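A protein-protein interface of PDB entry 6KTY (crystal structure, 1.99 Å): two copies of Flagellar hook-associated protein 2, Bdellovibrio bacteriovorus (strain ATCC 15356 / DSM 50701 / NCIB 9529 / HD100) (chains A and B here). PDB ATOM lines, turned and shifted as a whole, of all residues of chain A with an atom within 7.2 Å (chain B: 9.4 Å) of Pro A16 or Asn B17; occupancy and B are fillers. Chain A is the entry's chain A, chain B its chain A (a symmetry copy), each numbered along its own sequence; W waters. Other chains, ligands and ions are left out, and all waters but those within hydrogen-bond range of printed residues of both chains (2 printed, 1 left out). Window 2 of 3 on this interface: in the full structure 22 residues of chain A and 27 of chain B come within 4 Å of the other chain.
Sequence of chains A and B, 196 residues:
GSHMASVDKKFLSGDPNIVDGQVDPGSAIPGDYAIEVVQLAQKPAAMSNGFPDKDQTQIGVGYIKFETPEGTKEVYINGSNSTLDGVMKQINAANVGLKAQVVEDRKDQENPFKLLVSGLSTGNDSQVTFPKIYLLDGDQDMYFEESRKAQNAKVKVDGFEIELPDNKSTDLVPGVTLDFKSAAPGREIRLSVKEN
Of chain A, only Gly A14 (3.0 Å), Asp A15 (3.8 Å) and Pro A16 (3.6 Å) come within 4 Å of Asn B17.
Gly A14 touches just these residues of chain B: Asn B17 and Lys B181.
Asp A15 touches just one residue of chain B: Asn B17 (3.8 Å).
Asn A17 touches none of the printed residues of chain B.
Of the printed residues of chain A, Leu B40 touches Glu A188 (3.7 Å) and Arg A190 (3.4 Å).
Of the printed residues of chain A, Lys B181 touches Gly A14 (3.8 Å), Ile A189 (3.8 Å) and Arg A190 (3.0 Å).
Of the printed residues of chain A, Phe B180 touches Arg A190 (3.0 Å).
Of the printed residues of chain A, Ala B183 touches Arg A187 (2.8 Å) and Glu A188 (3.0 Å).
Ile B189 touches none of the printed residues of chain A.
The nearest residue of chain B that does not touch Pro A16 is Pro B16 (7.6 Å).
Of the 19 printed residues of chain A, 7 touch a printed residue of chain B.
Along chain A the printed residues that touch a printed residue of chain B span positions 14 to 190.
Of the 20 printed residues of chain B, 8 touch a printed residue of chain A.
Printed residues of chain B that touch a printed residue of chain A: Asn B17, Leu B40, Asp B179, Phe B180, Lys B181, Ser B182, Ala B183 and Ala B184.
Hydrophobic or aromatic side chains of chain B that line the printed part of chain A: Leu B40 and Ala B184.
ND2 of Asn B17 lies within hydrogen-bond range of O of Gly A14 (3.0 Å).
NH1 of Arg A187 sits at hydrogen-bond distance from OG of Ser B182 (3.1 Å).
The backbone carbonyl oxygen of Ala B183 sits at hydrogen-bond distance from the guanidinium group of Arg A187 (2.8 Å).
The backbone carbonyl oxygen (O) of Glu A188 sits at hydrogen-bond distance from the backbone NH (N) of Ala B183.
OD1 of Asp B179 lies within salt-bridge range of NH2 of Arg A190 (2.6 Å).
O of Phe B180 is in hydrogen-bond range of NE of Arg A190 (3.0 Å).
The backbone carbonyl oxygen of Lys B181 sits at hydrogen-bond distance from the backbone NH of Arg A190 (3.0 Å).
Gly A14 touches Asn B17, but with the chains exchanged Asn A17 does not touch Gly B14 (11.4 Å).
Gly A14 touches Lys B181, but with the chains exchanged Lys A181 does not touch Gly B14 (18.2 Å).
Asp A15 touches Asn B17, but with the chains exchanged Asn A17 does not touch Asp B15 (7.9 Å).
Ile A189 touches Lys B181, but with the chains exchanged Lys A181 does not touch Ile B189 (18.8 Å).
16 positions are printed for both chains.
The backbone NH of Asn A17 lies within hydrogen-bond range of the side-chain carboxylate of Asp A15 (2.9 Å).
The backbone carbonyl oxygen (O) of Ile B18 sits at hydrogen-bond distance from the backbone NH (N) of Lys B181.
N of Asp B179 is in hydrogen-bond range of O of Asp B20.
The backbone carbonyl oxygen (O) of Val B37 sits at hydrogen-bond distance from the backbone NH (N) of Ala B184 (2.7 Å).
OD2 of Asp B179 is in salt-bridge range of NZ of Lys B181, at 3.2 Å.
Among the printed residues, pairs that only touch across the chains: Glu A188 with Ser B182, Arg A190 with Leu B40, Arg A187 with Ala B184, Ile A189 with Ser B182, Pro A16 with Asn B17, Glu A188 with Leu B40, Asp A15 with Asn B17, Ile A189 with Lys B181 and Gly A14 with Lys B181.
Water W1 lies within hydrogen-bond range of the side-chain carboxylate of Asp A15 (2.4 Å), the guanidinium group of Arg A187 (2.7 Å), the backbone carbonyl oxygen of Asn B17 (2.9 Å) and the side-chain hydroxyl of Ser B182 (3.3 Å).
Water W2 lies within hydrogen-bond range of OE1 of Glu A188 and N of Leu B40.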
ATOM      1  N   LEU A  12      -8.875  17.137  22.497  1.00  0.00           N
ATOM      2  CA  LEU A  12      -7.867  16.101  22.173  1.00  0.00           C
ATOM      3  C   LEU A  12      -8.472  14.908  21.433  1.00  0.00           C
ATOM      4  O   LEU A  12      -9.542  14.421  21.801  1.00  0.00           O
ATOM      5  CB  LEU A  12      -7.187  15.614  23.450  1.00  0.00           C
ATOM      6  CG  LEU A  12      -6.355  16.659  24.194  1.00  0.00           C
ATOM      7  CD1 LEU A  12      -6.030  16.206  25.624  1.00  0.00           C
ATOM      8  CD2 LEU A  12      -5.084  16.966  23.394  1.00  0.00           C
ATOM      9  N   SER A  13      -7.798  14.484  20.364  1.00  0.00           N
ATOM     10  CA  SER A  13      -8.149  13.256  19.661  1.00  0.00           C
ATOM     11  C   SER A  13      -7.216  12.142  20.122  1.00  0.00           C
ATOM     12  O   SER A  13      -6.013  12.367  20.260  1.00  0.00           O
ATOM     13  CB  SER A  13      -8.022  13.454  18.144  1.00  0.00           C
ATOM     14  OG  SER A  13      -8.169  12.218  17.448  1.00  0.00           O
ATOM     15  N   GLY A  14      -7.780  10.956  20.387  1.00  0.00           N
ATOM     16  CA  GLY A  14      -6.990   9.768  20.672  1.00  0.00           C
ATOM     17  C   GLY A  14      -6.035   9.420  19.528  1.00  0.00           C
ATOM     18  O   GLY A  14      -4.996   8.828  19.762  1.00  0.00           O
ATOM     19  N   ASP A  15      -6.398   9.775  18.296  1.00  0.00           N
ATOM     20  CA  ASP A  15      -5.485   9.619  17.154  1.00  0.00           C
ATOM     21  C   ASP A  15      -5.645  10.732  16.140  1.00  0.00           C
ATOM     22  O   ASP A  15      -6.514  10.666  15.267  1.00  0.00           O
ATOM     23  CB  ASP A  15      -5.659   8.263  16.471  1.00  0.00           C
ATOM     24  CG  ASP A  15      -4.485   7.927  15.548  1.00  0.00           C
ATOM     25  OD1 ASP A  15      -3.818   8.871  15.042  1.00  0.00           O
ATOM     26  OD2 ASP A  15      -4.221   6.718  15.365  1.00  0.00           O
ATOM     27  N   PRO A  16      -4.771  11.747  16.227  1.00  0.00           N
ATOM     28  CA  PRO A  16      -4.855  12.889  15.297  1.00  0.00           C
ATOM     29  C   PRO A  16      -4.629  12.518  13.836  1.00  0.00           C
ATOM     30  O   PRO A  16      -4.970  13.300  12.955  1.00  0.00           O
ATOM     31  CB  PRO A  16      -3.744  13.848  15.788  1.00  0.00           C
ATOM     32  CG  PRO A  16      -3.363  13.386  17.146  1.00  0.00           C
ATOM     33  CD  PRO A  16      -3.707  11.917  17.237  1.00  0.00           C
ATOM     34  N   ASN A  17      -4.069  11.337  13.570  1.00  0.00           N
ATOM     35  CA  ASN A  17      -3.837  10.888  12.191  1.00  0.00           C
ATOM     36  C   ASN A  17      -5.035  10.117  11.627  1.00  0.00           C
ATOM     37  O   ASN A  17      -4.981   9.601  10.503  1.00  0.00           O
ATOM     38  CB  ASN A  17      -2.592  10.017  12.134  1.00  0.00           C
ATOM     39  CG  ASN A  17      -1.331  10.785  12.543  1.00  0.00           C
ATOM     40  OD1 ASN A  17      -0.631  10.376  13.443  1.00  0.00           O
ATOM     41  ND2 ASN A  17      -1.079  11.906  11.898  1.00  0.00           N
ATOM     42  N   ILE A  18      -6.104  10.033  12.411  1.00  0.00           N
ATOM     43  CA  ILE A  18      -7.393   9.552  11.900  1.00  0.00           C
ATOM     44  C   ILE A  18      -8.420  10.664  11.933  1.00  0.00           C
ATOM     45  O   ILE A  18      -9.083  10.952  10.916  1.00  0.00           O
ATOM     46  CB  ILE A  18      -7.911   8.265  12.621  1.00  0.00           C
ATOM     47  CG1 ILE A  18      -6.926   7.116  12.402  1.00  0.00           C
ATOM     48  CG2 ILE A  18      -9.321   7.885  12.081  1.00  0.00           C
ATOM     49  CD1 ILE A  18      -7.252   5.810  13.170  1.00  0.00           C
ATOM     50  N   VAL A  19      -8.559  11.308  13.091  1.00  0.00           N
ATOM     51  CA  VAL A  19      -9.458  12.441  13.221  1.00  0.00           C
ATOM     52  C   VAL A  19      -8.767  13.498  14.067  1.00  0.00           C
ATOM     53  O   VAL A  19      -8.232  13.177  15.113  1.00  0.00           O
ATOM     54  CB  VAL A  19     -10.775  12.037  13.909  1.00  0.00           C
ATOM     55  CG1 VAL A  19     -11.709  13.251  13.938  1.00  0.00           C
ATOM     56  CG2 VAL A  19     -11.441  10.894  13.184  1.00  0.00           C
ATOM     57  N   ASP A  20      -8.744  14.748  13.608  1.00  0.00           N
ATOM     58  CA  ASP A  20      -8.262  15.838  14.449  1.00  0.00           C
ATOM     59  C   ASP A  20      -9.298  16.949  14.372  1.00  0.00           C
ATOM     60  O   ASP A  20     -10.333  16.804  13.694  1.00  0.00           O
ATOM     61  CB  ASP A  20      -6.881  16.350  13.994  1.00  0.00           C
ATOM     62  CG  ASP A  20      -6.068  16.959  15.133  1.00  0.00           C
ATOM     63  OD1 ASP A  20      -6.605  17.191  16.232  1.00  0.00           O
ATOM     64  OD2 ASP A  20      -4.876  17.211  14.937  1.00  0.00           O
ATOM     65  N   GLY A  21      -9.043  18.041  15.087  1.00  0.00           N
ATOM     66  CA  GLY A  21      -9.989  19.131  15.134  1.00  0.00           C
ATOM     67  C   GLY A  21      -9.524  20.296  15.970  1.00  0.00           C
ATOM     68  O   GLY A  21      -8.444  20.258  16.559  1.00  0.00           O
ATOM     69  N   ASP A 179     -11.747  17.381  11.279  1.00  0.00           N
ATOM     70  CA  ASP A 179     -11.252  17.024   9.959  1.00  0.00           C
ATOM     71  C   ASP A 179     -10.826  15.561   9.971  1.00  0.00           C
ATOM     72  O   ASP A 179      -9.976  15.162  10.784  1.00  0.00           O
ATOM     73  CB  ASP A 179     -10.063  17.923   9.579  1.00  0.00           C
ATOM     74  CG  ASP A 179      -9.725  17.851   8.091  1.00  0.00           C
ATOM     75  OD1 ASP A 179     -10.635  18.106   7.239  1.00  0.00           O
ATOM     76  OD2 ASP A 179      -8.543  17.557   7.756  1.00  0.00           O
ATOM     77  N   PHE A 180     -11.417  14.750   9.085  1.00  0.00           N
ATOM     78  CA  PHE A 180     -11.019  13.352   8.986  1.00  0.00           C
ATOM     79  C   PHE A 180      -9.709  13.258   8.198  1.00  0.00           C
ATOM     80  O   PHE A 180      -9.646  13.683   7.024  1.00  0.00           O
ATOM     81  CB  PHE A 180     -12.132  12.503   8.337  1.00  0.00           C
ATOM     82  CG  PHE A 180     -13.487  12.798   8.886  1.00  0.00           C
ATOM     83  CD1 PHE A 180     -13.674  12.958  10.253  1.00  0.00           C
ATOM     84  CD2 PHE A 180     -14.581  12.939   8.049  1.00  0.00           C
ATOM     85  CE1 PHE A 180     -14.930  13.252  10.777  1.00  0.00           C
ATOM     86  CE2 PHE A 180     -15.826  13.246   8.562  1.00  0.00           C
ATOM     87  CZ  PHE A 180     -15.996  13.418   9.932  1.00  0.00           C
ATOM     88  N   LYS A 181      -8.675  12.703   8.825  1.00  0.00           N
ATOM     89  CA  LYS A 181      -7.344  12.597   8.172  1.00  0.00           C
ATOM     90  C   LYS A 181      -7.123  11.285   7.403  1.00  0.00           C
ATOM     91  O   LYS A 181      -6.286  11.217   6.498  1.00  0.00           O
ATOM     92  CB  LYS A 181      -6.265  12.728   9.203  1.00  0.00           C
ATOM     93  CG  LYS A 181      -6.355  13.907  10.128  1.00  0.00           C
ATOM     94  CD  LYS A 181      -6.216  15.176   9.376  1.00  0.00           C
ATOM     95  CE  LYS A 181      -5.937  16.321  10.302  1.00  0.00           C
ATOM     96  NZ  LYS A 181      -5.895  17.599   9.550  1.00  0.00           N
ATOM     97  N   SER A 182      -7.818  10.230   7.798  1.00  0.00           N
ATOM     98  CA  SER A 182      -7.717   8.927   7.140  1.00  0.00           C
ATOM     99  C   SER A 182      -8.921   8.091   7.458  1.00  0.00           C
ATOM    100  O   SER A 182      -9.580   8.338   8.446  1.00  0.00           O
ATOM    101  CB  SER A 182      -6.419   8.192   7.583  1.00  0.00           C
ATOM    102  OG  SER A 182      -6.394   7.921   8.979  1.00  0.00           O
ATOM    103  N   ARG A 187     -11.586   0.946  13.709  1.00  0.00           N
ATOM    104  CA  ARG A 187     -10.693   1.626  14.631  1.00  0.00           C
ATOM    105  C   ARG A 187     -11.422   2.853  15.219  1.00  0.00           C
ATOM    106  O   ARG A 187     -11.177   4.033  14.845  1.00  0.00           O
ATOM    107  CB  ARG A 187      -9.409   2.059  13.919  1.00  0.00           C
ATOM    108  CG  ARG A 187      -8.602   0.910  13.250  1.00  0.00           C
ATOM    109  CD  ARG A 187      -7.537   0.269  14.121  1.00  0.00           C
ATOM    110  NE  ARG A 187      -6.329   1.098  14.216  1.00  0.00           N
ATOM    111  CZ  ARG A 187      -6.071   1.971  15.185  1.00  0.00           C
ATOM    112  NH1 ARG A 187      -6.894   2.128  16.224  1.00  0.00           N
ATOM    113  NH2 ARG A 187      -4.956   2.680  15.143  1.00  0.00           N
ATOM    114  N   GLU A 188     -12.293   2.570  16.170  1.00  0.00           N
ATOM    115  CA  GLU A 188     -12.989   3.593  16.899  1.00  0.00           C
ATOM    116  C   GLU A 188     -11.980   4.408  17.713  1.00  0.00           C
ATOM    117  O   GLU A 188     -11.083   3.842  18.391  1.00  0.00           O
ATOM    118  CB  GLU A 188     -14.072   2.970  17.790  1.00  0.00           C
ATOM    119  CG  GLU A 188     -15.082   3.970  18.316  1.00  0.00           C
ATOM    120  CD  GLU A 188     -16.247   3.318  19.068  1.00  0.00           C
ATOM    121  OE1 GLU A 188     -16.034   2.280  19.730  1.00  0.00           O
ATOM    122  OE2 GLU A 188     -17.388   3.874  19.024  1.00  0.00           O
ATOM    123  N   ILE A 189     -12.102   5.723  17.620  1.00  0.00           N
ATOM    124  CA  ILE A 189     -11.181   6.684  18.269  1.00  0.00           C
ATOM    125  C   ILE A 189     -11.987   7.381  19.363  1.00  0.00           C
ATOM    126  O   ILE A 189     -13.179   7.712  19.163  1.00  0.00           O
ATOM    127  CB  ILE A 189     -10.678   7.783  17.298  1.00  0.00           C
ATOM    128  CG1 ILE A 189     -10.078   7.190  16.005  1.00  0.00           C
ATOM    129  CG2 ILE A 189      -9.676   8.696  17.959  1.00  0.00           C
ATOM    130  CD1 ILE A 189      -9.290   5.947  16.202  1.00  0.00           C
ATOM    131  N   ARG A 190     -11.352   7.611  20.513  1.00  0.00           N
ATOM    132  CA  ARG A 190     -11.967   8.406  21.555  1.00  0.00           C
ATOM    133  C   ARG A 190     -11.434   9.851  21.502  1.00  0.00           C
ATOM    134  O   ARG A 190     -10.247  10.059  21.367  1.00  0.00           O
ATOM    135  CB  ARG A 190     -11.703   7.790  22.930  1.00  0.00           C
ATOM    136  CG  ARG A 190     -12.521   6.532  23.224  1.00  0.00           C
ATOM    137  CD  ARG A 190     -12.868   6.469  24.714  1.00  0.00           C
ATOM    138  NE  ARG A 190     -11.649   6.626  25.475  1.00  0.00           N
ATOM    139  CZ  ARG A 190     -11.516   7.242  26.641  1.00  0.00           C
ATOM    140  NH1 ARG A 190     -12.532   7.808  27.276  1.00  0.00           N
ATOM    141  NH2 ARG A 190     -10.316   7.291  27.176  1.00  0.00           N
ATOM    142  N   LEU A 191     -12.351  10.815  21.572  1.00  0.00           N
ATOM    143  CA  LEU A 191     -12.054  12.231  21.517  1.00  0.00           C
ATOM    144  C   LEU A 191     -12.542  12.837  22.832  1.00  0.00           C
ATOM    145  O   LEU A 191     -13.543  12.385  23.386  1.00  0.00           O
ATOM    146  CB  LEU A 191     -12.850  12.870  20.396  1.00  0.00           C
ATOM    147  CG  LEU A 191     -12.491  12.671  18.911  1.00  0.00           C
ATOM    148  CD1 LEU A 191     -11.511  11.599  18.614  1.00  0.00           C
ATOM    149  CD2 LEU A 191     -13.751  12.466  18.107  1.00  0.00           C
ATOM    150  N   SER B  13       4.355   3.739  26.334  1.00  0.00           N
ATOM    151  CA  SER B  13       3.513   2.901  25.489  1.00  0.00           C
ATOM    152  C   SER B  13       4.142   2.810  24.104  1.00  0.00           C
ATOM    153  O   SER B  13       4.613   3.818  23.576  1.00  0.00           O
ATOM    154  CB  SER B  13       2.101   3.495  25.386  1.00  0.00           C
ATOM    155  OG  SER B  13       1.319   2.804  24.414  1.00  0.00           O
ATOM    156  N   GLY B  14       4.175   1.597  23.536  1.00  0.00           N
ATOM    157  CA  GLY B  14       4.593   1.397  22.157  1.00  0.00           C
ATOM    158  C   GLY B  14       3.731   2.188  21.171  1.00  0.00           C
ATOM    159  O   GLY B  14       4.202   2.551  20.108  1.00  0.00           O
ATOM    160  N   ASP B  15       2.469   2.438  21.521  1.00  0.00           N
ATOM    161  CA  ASP B  15       1.610   3.313  20.713  1.00  0.00           C
ATOM    162  C   ASP B  15       0.657   4.124  21.566  1.00  0.00           C
ATOM    163  O   ASP B  15      -0.421   3.647  21.930  1.00  0.00           O
ATOM    164  CB  ASP B  15       0.827   2.526  19.662  1.00  0.00           C
ATOM    165  CG  ASP B  15       0.237   3.435  18.581  1.00  0.00           C
ATOM    166  OD1 ASP B  15      -0.014   4.638  18.865  1.00  0.00           O
ATOM    167  OD2 ASP B  15       0.062   2.943  17.444  1.00  0.00           O
ATOM    168  N   PRO B  16       1.036   5.378  21.854  1.00  0.00           N
ATOM    169  CA  PRO B  16       0.187   6.243  22.696  1.00  0.00           C
ATOM    170  C   PRO B  16      -1.178   6.550  22.091  1.00  0.00           C
ATOM    171  O   PRO B  16      -2.071   6.989  22.808  1.00  0.00           O
ATOM    172  CB  PRO B  16       1.015   7.541  22.846  1.00  0.00           C
ATOM    173  CG  PRO B  16       2.395   7.209  22.416  1.00  0.00           C
ATOM    174  CD  PRO B  16       2.304   6.033  21.472  1.00  0.00           C
ATOM    175  N   ASN B  17      -1.351   6.318  20.789  1.00  0.00           N
ATOM    176  CA  ASN B  17      -2.641   6.562  20.128  1.00  0.00           C
ATOM    177  C   ASN B  17      -3.551   5.331  20.169  1.00  0.00           C
ATOM    178  O   ASN B  17      -4.647   5.336  19.594  1.00  0.00           O
ATOM    179  CB  ASN B  17      -2.411   6.982  18.685  1.00  0.00           C
ATOM    180  CG  ASN B  17      -1.632   8.298  18.585  1.00  0.00           C
ATOM    181  OD1 ASN B  17      -0.602   8.352  17.950  1.00  0.00           O
ATOM    182  ND2 ASN B  17      -2.118   9.332  19.242  1.00  0.00           N
ATOM    183  N   ILE B  18      -3.091   4.279  20.839  1.00  0.00           N
ATOM    184  CA  ILE B  18      -3.959   3.143  21.171  1.00  0.00           C
ATOM    185  C   ILE B  18      -4.139   3.039  22.671  1.00  0.00           C
ATOM    186  O   ILE B  18      -5.279   2.968  23.174  1.00  0.00           O
ATOM    187  CB  ILE B  18      -3.481   1.789  20.552  1.00  0.00           C
ATOM    188  CG1 ILE B  18      -3.493   1.885  19.026  1.00  0.00           C
ATOM    189  CG2 ILE B  18      -4.404   0.631  21.032  1.00  0.00           C
ATOM    190  CD1 ILE B  18      -2.919   0.654  18.281  1.00  0.00           C
ATOM    191  N   VAL B  19      -3.026   3.039  23.404  1.00  0.00           N
ATOM    192  CA  VAL B  19      -3.078   3.021  24.854  1.00  0.00           C
ATOM    193  C   VAL B  19      -2.017   3.975  25.377  1.00  0.00           C
ATOM    194  O   VAL B  19      -0.885   3.922  24.929  1.00  0.00           O
ATOM    195  CB  VAL B  19      -2.796   1.612  25.408  1.00  0.00           C
ATOM    196  CG1 VAL B  19      -2.949   1.641  26.933  1.00  0.00           C
ATOM    197  CG2 VAL B  19      -3.739   0.594  24.817  1.00  0.00           C
ATOM    198  N   ASP B  20      -2.378   4.868  26.297  1.00  0.00           N
ATOM    199  CA  ASP B  20      -1.376   5.686  26.970  1.00  0.00           C
ATOM    200  C   ASP B  20      -1.665   5.602  28.462  1.00  0.00           C
ATOM    201  O   ASP B  20      -2.604   4.903  28.886  1.00  0.00           O
ATOM    202  CB  ASP B  20      -1.410   7.151  26.491  1.00  0.00           C
ATOM    203  CG  ASP B  20      -0.060   7.851  26.622  1.00  0.00           C
ATOM    204  OD1 ASP B  20       0.864   7.314  27.260  1.00  0.00           O
ATOM    205  OD2 ASP B  20       0.088   8.951  26.082  1.00  0.00           O
ATOM    206  N   GLY B  21      -0.845   6.282  29.258  1.00  0.00           N
ATOM    207  CA  GLY B  21      -0.991   6.222  30.694  1.00  0.00           C
ATOM    208  C   GLY B  21       0.006   7.075  31.436  1.00  0.00           C
ATOM    209  O   GLY B  21       0.861   7.718  30.829  1.00  0.00           O
ATOM    210  N   VAL B  37      -6.134  -3.546  22.737  1.00  0.00           N
ATOM    211  CA  VAL B  37      -7.498  -3.018  22.892  1.00  0.00           C
ATOM    212  C   VAL B  37      -8.375  -3.581  21.771  1.00  0.00           C
ATOM    213  O   VAL B  37      -8.257  -3.160  20.604  1.00  0.00           O
ATOM    214  CB  VAL B  37      -7.527  -1.507  22.854  1.00  0.00           C
ATOM    215  CG1 VAL B  37      -8.986  -1.025  23.169  1.00  0.00           C
ATOM    216  CG2 VAL B  37      -6.511  -0.949  23.794  1.00  0.00           C
ATOM    217  N   LEU B  40     -13.460  -0.701  22.431  1.00  0.00           N
ATOM    218  CA  LEU B  40     -13.641   0.275  23.480  1.00  0.00           C
ATOM    219  C   LEU B  40     -14.918  -0.061  24.254  1.00  0.00           C
ATOM    220  O   LEU B  40     -15.822  -0.711  23.739  1.00  0.00           O
ATOM    221  CB  LEU B  40     -13.737   1.686  22.917  1.00  0.00           C
ATOM    222  CG  LEU B  40     -12.481   2.227  22.236  1.00  0.00           C
ATOM    223  CD1 LEU B  40     -12.847   3.565  21.608  1.00  0.00           C
ATOM    224  CD2 LEU B  40     -11.279   2.410  23.187  1.00  0.00           C
ATOM    225  N   ASP B 179      -5.273   4.791  29.900  1.00  0.00           N
ATOM    226  CA  ASP B 179      -6.430   5.274  29.162  1.00  0.00           C
ATOM    227  C   ASP B 179      -6.388   4.701  27.751  1.00  0.00           C
ATOM    228  O   ASP B 179      -5.400   4.895  27.023  1.00  0.00           O
ATOM    229  CB  ASP B 179      -6.420   6.812  29.113  1.00  0.00           C
ATOM    230  CG  ASP B 179      -7.763   7.392  28.674  1.00  0.00           C
ATOM    231  OD1 ASP B 179      -8.814   7.074  29.319  1.00  0.00           O
ATOM    232  OD2 ASP B 179      -7.784   8.186  27.692  1.00  0.00           O
ATOM    233  N   PHE B 180      -7.447   3.982  27.358  1.00  0.00           N
ATOM    234  CA  PHE B 180      -7.517   3.454  26.002  1.00  0.00           C
ATOM    235  C   PHE B 180      -7.925   4.579  25.046  1.00  0.00           C
ATOM    236  O   PHE B 180      -9.011   5.177  25.203  1.00  0.00           O
ATOM    237  CB  PHE B 180      -8.490   2.260  25.920  1.00  0.00           C
ATOM    238  CG  PHE B 180      -8.312   1.283  27.033  1.00  0.00           C
ATOM    239  CD1 PHE B 180      -7.039   0.900  27.436  1.00  0.00           C
ATOM    240  CD2 PHE B 180      -9.403   0.754  27.700  1.00  0.00           C
ATOM    241  CE1 PHE B 180      -6.857   0.003  28.486  1.00  0.00           C
ATOM    242  CE2 PHE B 180      -9.228  -0.124  28.752  1.00  0.00           C
ATOM    243  CZ  PHE B 180      -7.947  -0.487  29.155  1.00  0.00           C
ATOM    244  N   LYS B 181      -7.076   4.864  24.062  1.00  0.00           N
ATOM    245  CA  LYS B 181      -7.350   5.963  23.101  1.00  0.00           C
ATOM    246  C   LYS B 181      -8.106   5.521  21.838  1.00  0.00           C
ATOM    247  O   LYS B 181      -8.754   6.334  21.172  1.00  0.00           O
ATOM    248  CB  LYS B 181      -6.060   6.599  22.680  1.00  0.00           C
ATOM    249  CG  LYS B 181      -5.127   7.019  23.778  1.00  0.00           C
ATOM    250  CD  LYS B 181      -5.737   8.084  24.607  1.00  0.00           C
ATOM    251  CE  LYS B 181      -4.705   8.762  25.457  1.00  0.00           C
ATOM    252  NZ  LYS B 181      -5.342   9.759  26.352  1.00  0.00           N
ATOM    253  N   SER B 182      -7.976   4.257  21.468  1.00  0.00           N
ATOM    254  CA  SER B 182      -8.657   3.702  20.299  1.00  0.00           C
ATOM    255  C   SER B 182      -8.726   2.207  20.398  1.00  0.00           C
ATOM    256  O   SER B 182      -7.940   1.615  21.108  1.00  0.00           O
ATOM    257  CB  SER B 182      -7.925   4.121  18.991  1.00  0.00           C
ATOM    258  OG  SER B 182      -6.592   3.627  18.930  1.00  0.00           O
ATOM    259  N   ALA B 183      -9.657   1.592  19.678  1.00  0.00           N
ATOM    260  CA  ALA B 183      -9.741   0.138  19.561  1.00  0.00           C
ATOM    261  C   ALA B 183      -8.847  -0.280  18.398  1.00  0.00           C
ATOM    262  O   ALA B 183      -8.823   0.371  17.369  1.00  0.00           O
ATOM    263  CB  ALA B 183     -11.165  -0.288  19.294  1.00  0.00           C
ATOM    264  N   ALA B 184      -8.075  -1.345  18.562  1.00  0.00           N
ATOM    265  CA  ALA B 184      -7.237  -1.784  17.440  1.00  0.00           C
ATOM    266  C   ALA B 184      -7.101  -3.273  17.496  1.00  0.00           C
ATOM    267  O   ALA B 184      -6.077  -3.799  17.939  1.00  0.00           O
ATOM    268  CB  ALA B 184      -5.894  -1.090  17.467  1.00  0.00           C
ATOM    269  N   ARG B 187      -3.857  -5.708  17.101  1.00  0.00           N
ATOM    270  CA  ARG B 187      -2.690  -4.851  17.215  1.00  0.00           C
ATOM    271  C   ARG B 187      -2.249  -4.798  18.693  1.00  0.00           C
ATOM    272  O   ARG B 187      -2.474  -3.801  19.434  1.00  0.00           O
ATOM    273  CB  ARG B 187      -3.002  -3.443  16.700  1.00  0.00           C
ATOM    274  CG  ARG B 187      -3.495  -3.370  15.227  1.00  0.00           C
ATOM    275  CD  ARG B 187      -2.407  -3.175  14.186  1.00  0.00           C
ATOM    276  NE  ARG B 187      -1.940  -1.784  14.128  1.00  0.00           N
ATOM    277  CZ  ARG B 187      -0.888  -1.298  14.780  1.00  0.00           C
ATOM    278  NH1 ARG B 187      -0.103  -2.081  15.523  1.00  0.00           N
ATOM    279  NH2 ARG B 187      -0.587  -0.016  14.666  1.00  0.00           N
ATOM    280  N   ILE B 189       0.043  -4.158  21.660  1.00  0.00           N
ATOM    281  CA  ILE B 189       0.971  -3.040  21.945  1.00  0.00           C
ATOM    282  C   ILE B 189       1.846  -3.495  23.112  1.00  0.00           C
ATOM    283  O   ILE B 189       1.351  -4.140  24.065  1.00  0.00           O
ATOM    284  CB  ILE B 189       0.238  -1.750  22.395  1.00  0.00           C
ATOM    285  CG1 ILE B 189      -0.877  -1.339  21.410  1.00  0.00           C
ATOM    286  CG2 ILE B 189       1.198  -0.604  22.595  1.00  0.00           C
ATOM    287  CD1 ILE B 189      -0.548  -1.552  19.978  1.00  0.00           C
ATOM    288  N   LEU B 191       4.071  -2.225  26.312  1.00  0.00           N
ATOM    289  CA  LEU B 191       4.182  -1.125  27.246  1.00  0.00           C
ATOM    290  C   LEU B 191       5.349  -1.449  28.177  1.00  0.00           C
ATOM    291  O   LEU B 191       5.585  -2.617  28.487  1.00  0.00           O
ATOM    292  CB  LEU B 191       2.927  -1.056  28.094  1.00  0.00           C
ATOM    293  CG  LEU B 191       1.585  -0.537  27.543  1.00  0.00           C
ATOM    294  CD1 LEU B 191       1.502  -0.379  26.070  1.00  0.00           C
ATOM    295  CD2 LEU B 191       0.460  -1.411  28.040  1.00  0.00           C
HETATM  296  O   HOH W   1      -4.358   4.762  16.803  1.00  0.00           O
HETATM  297  O   HOH W   2     -14.500   0.017  19.948  1.00  0.00           O
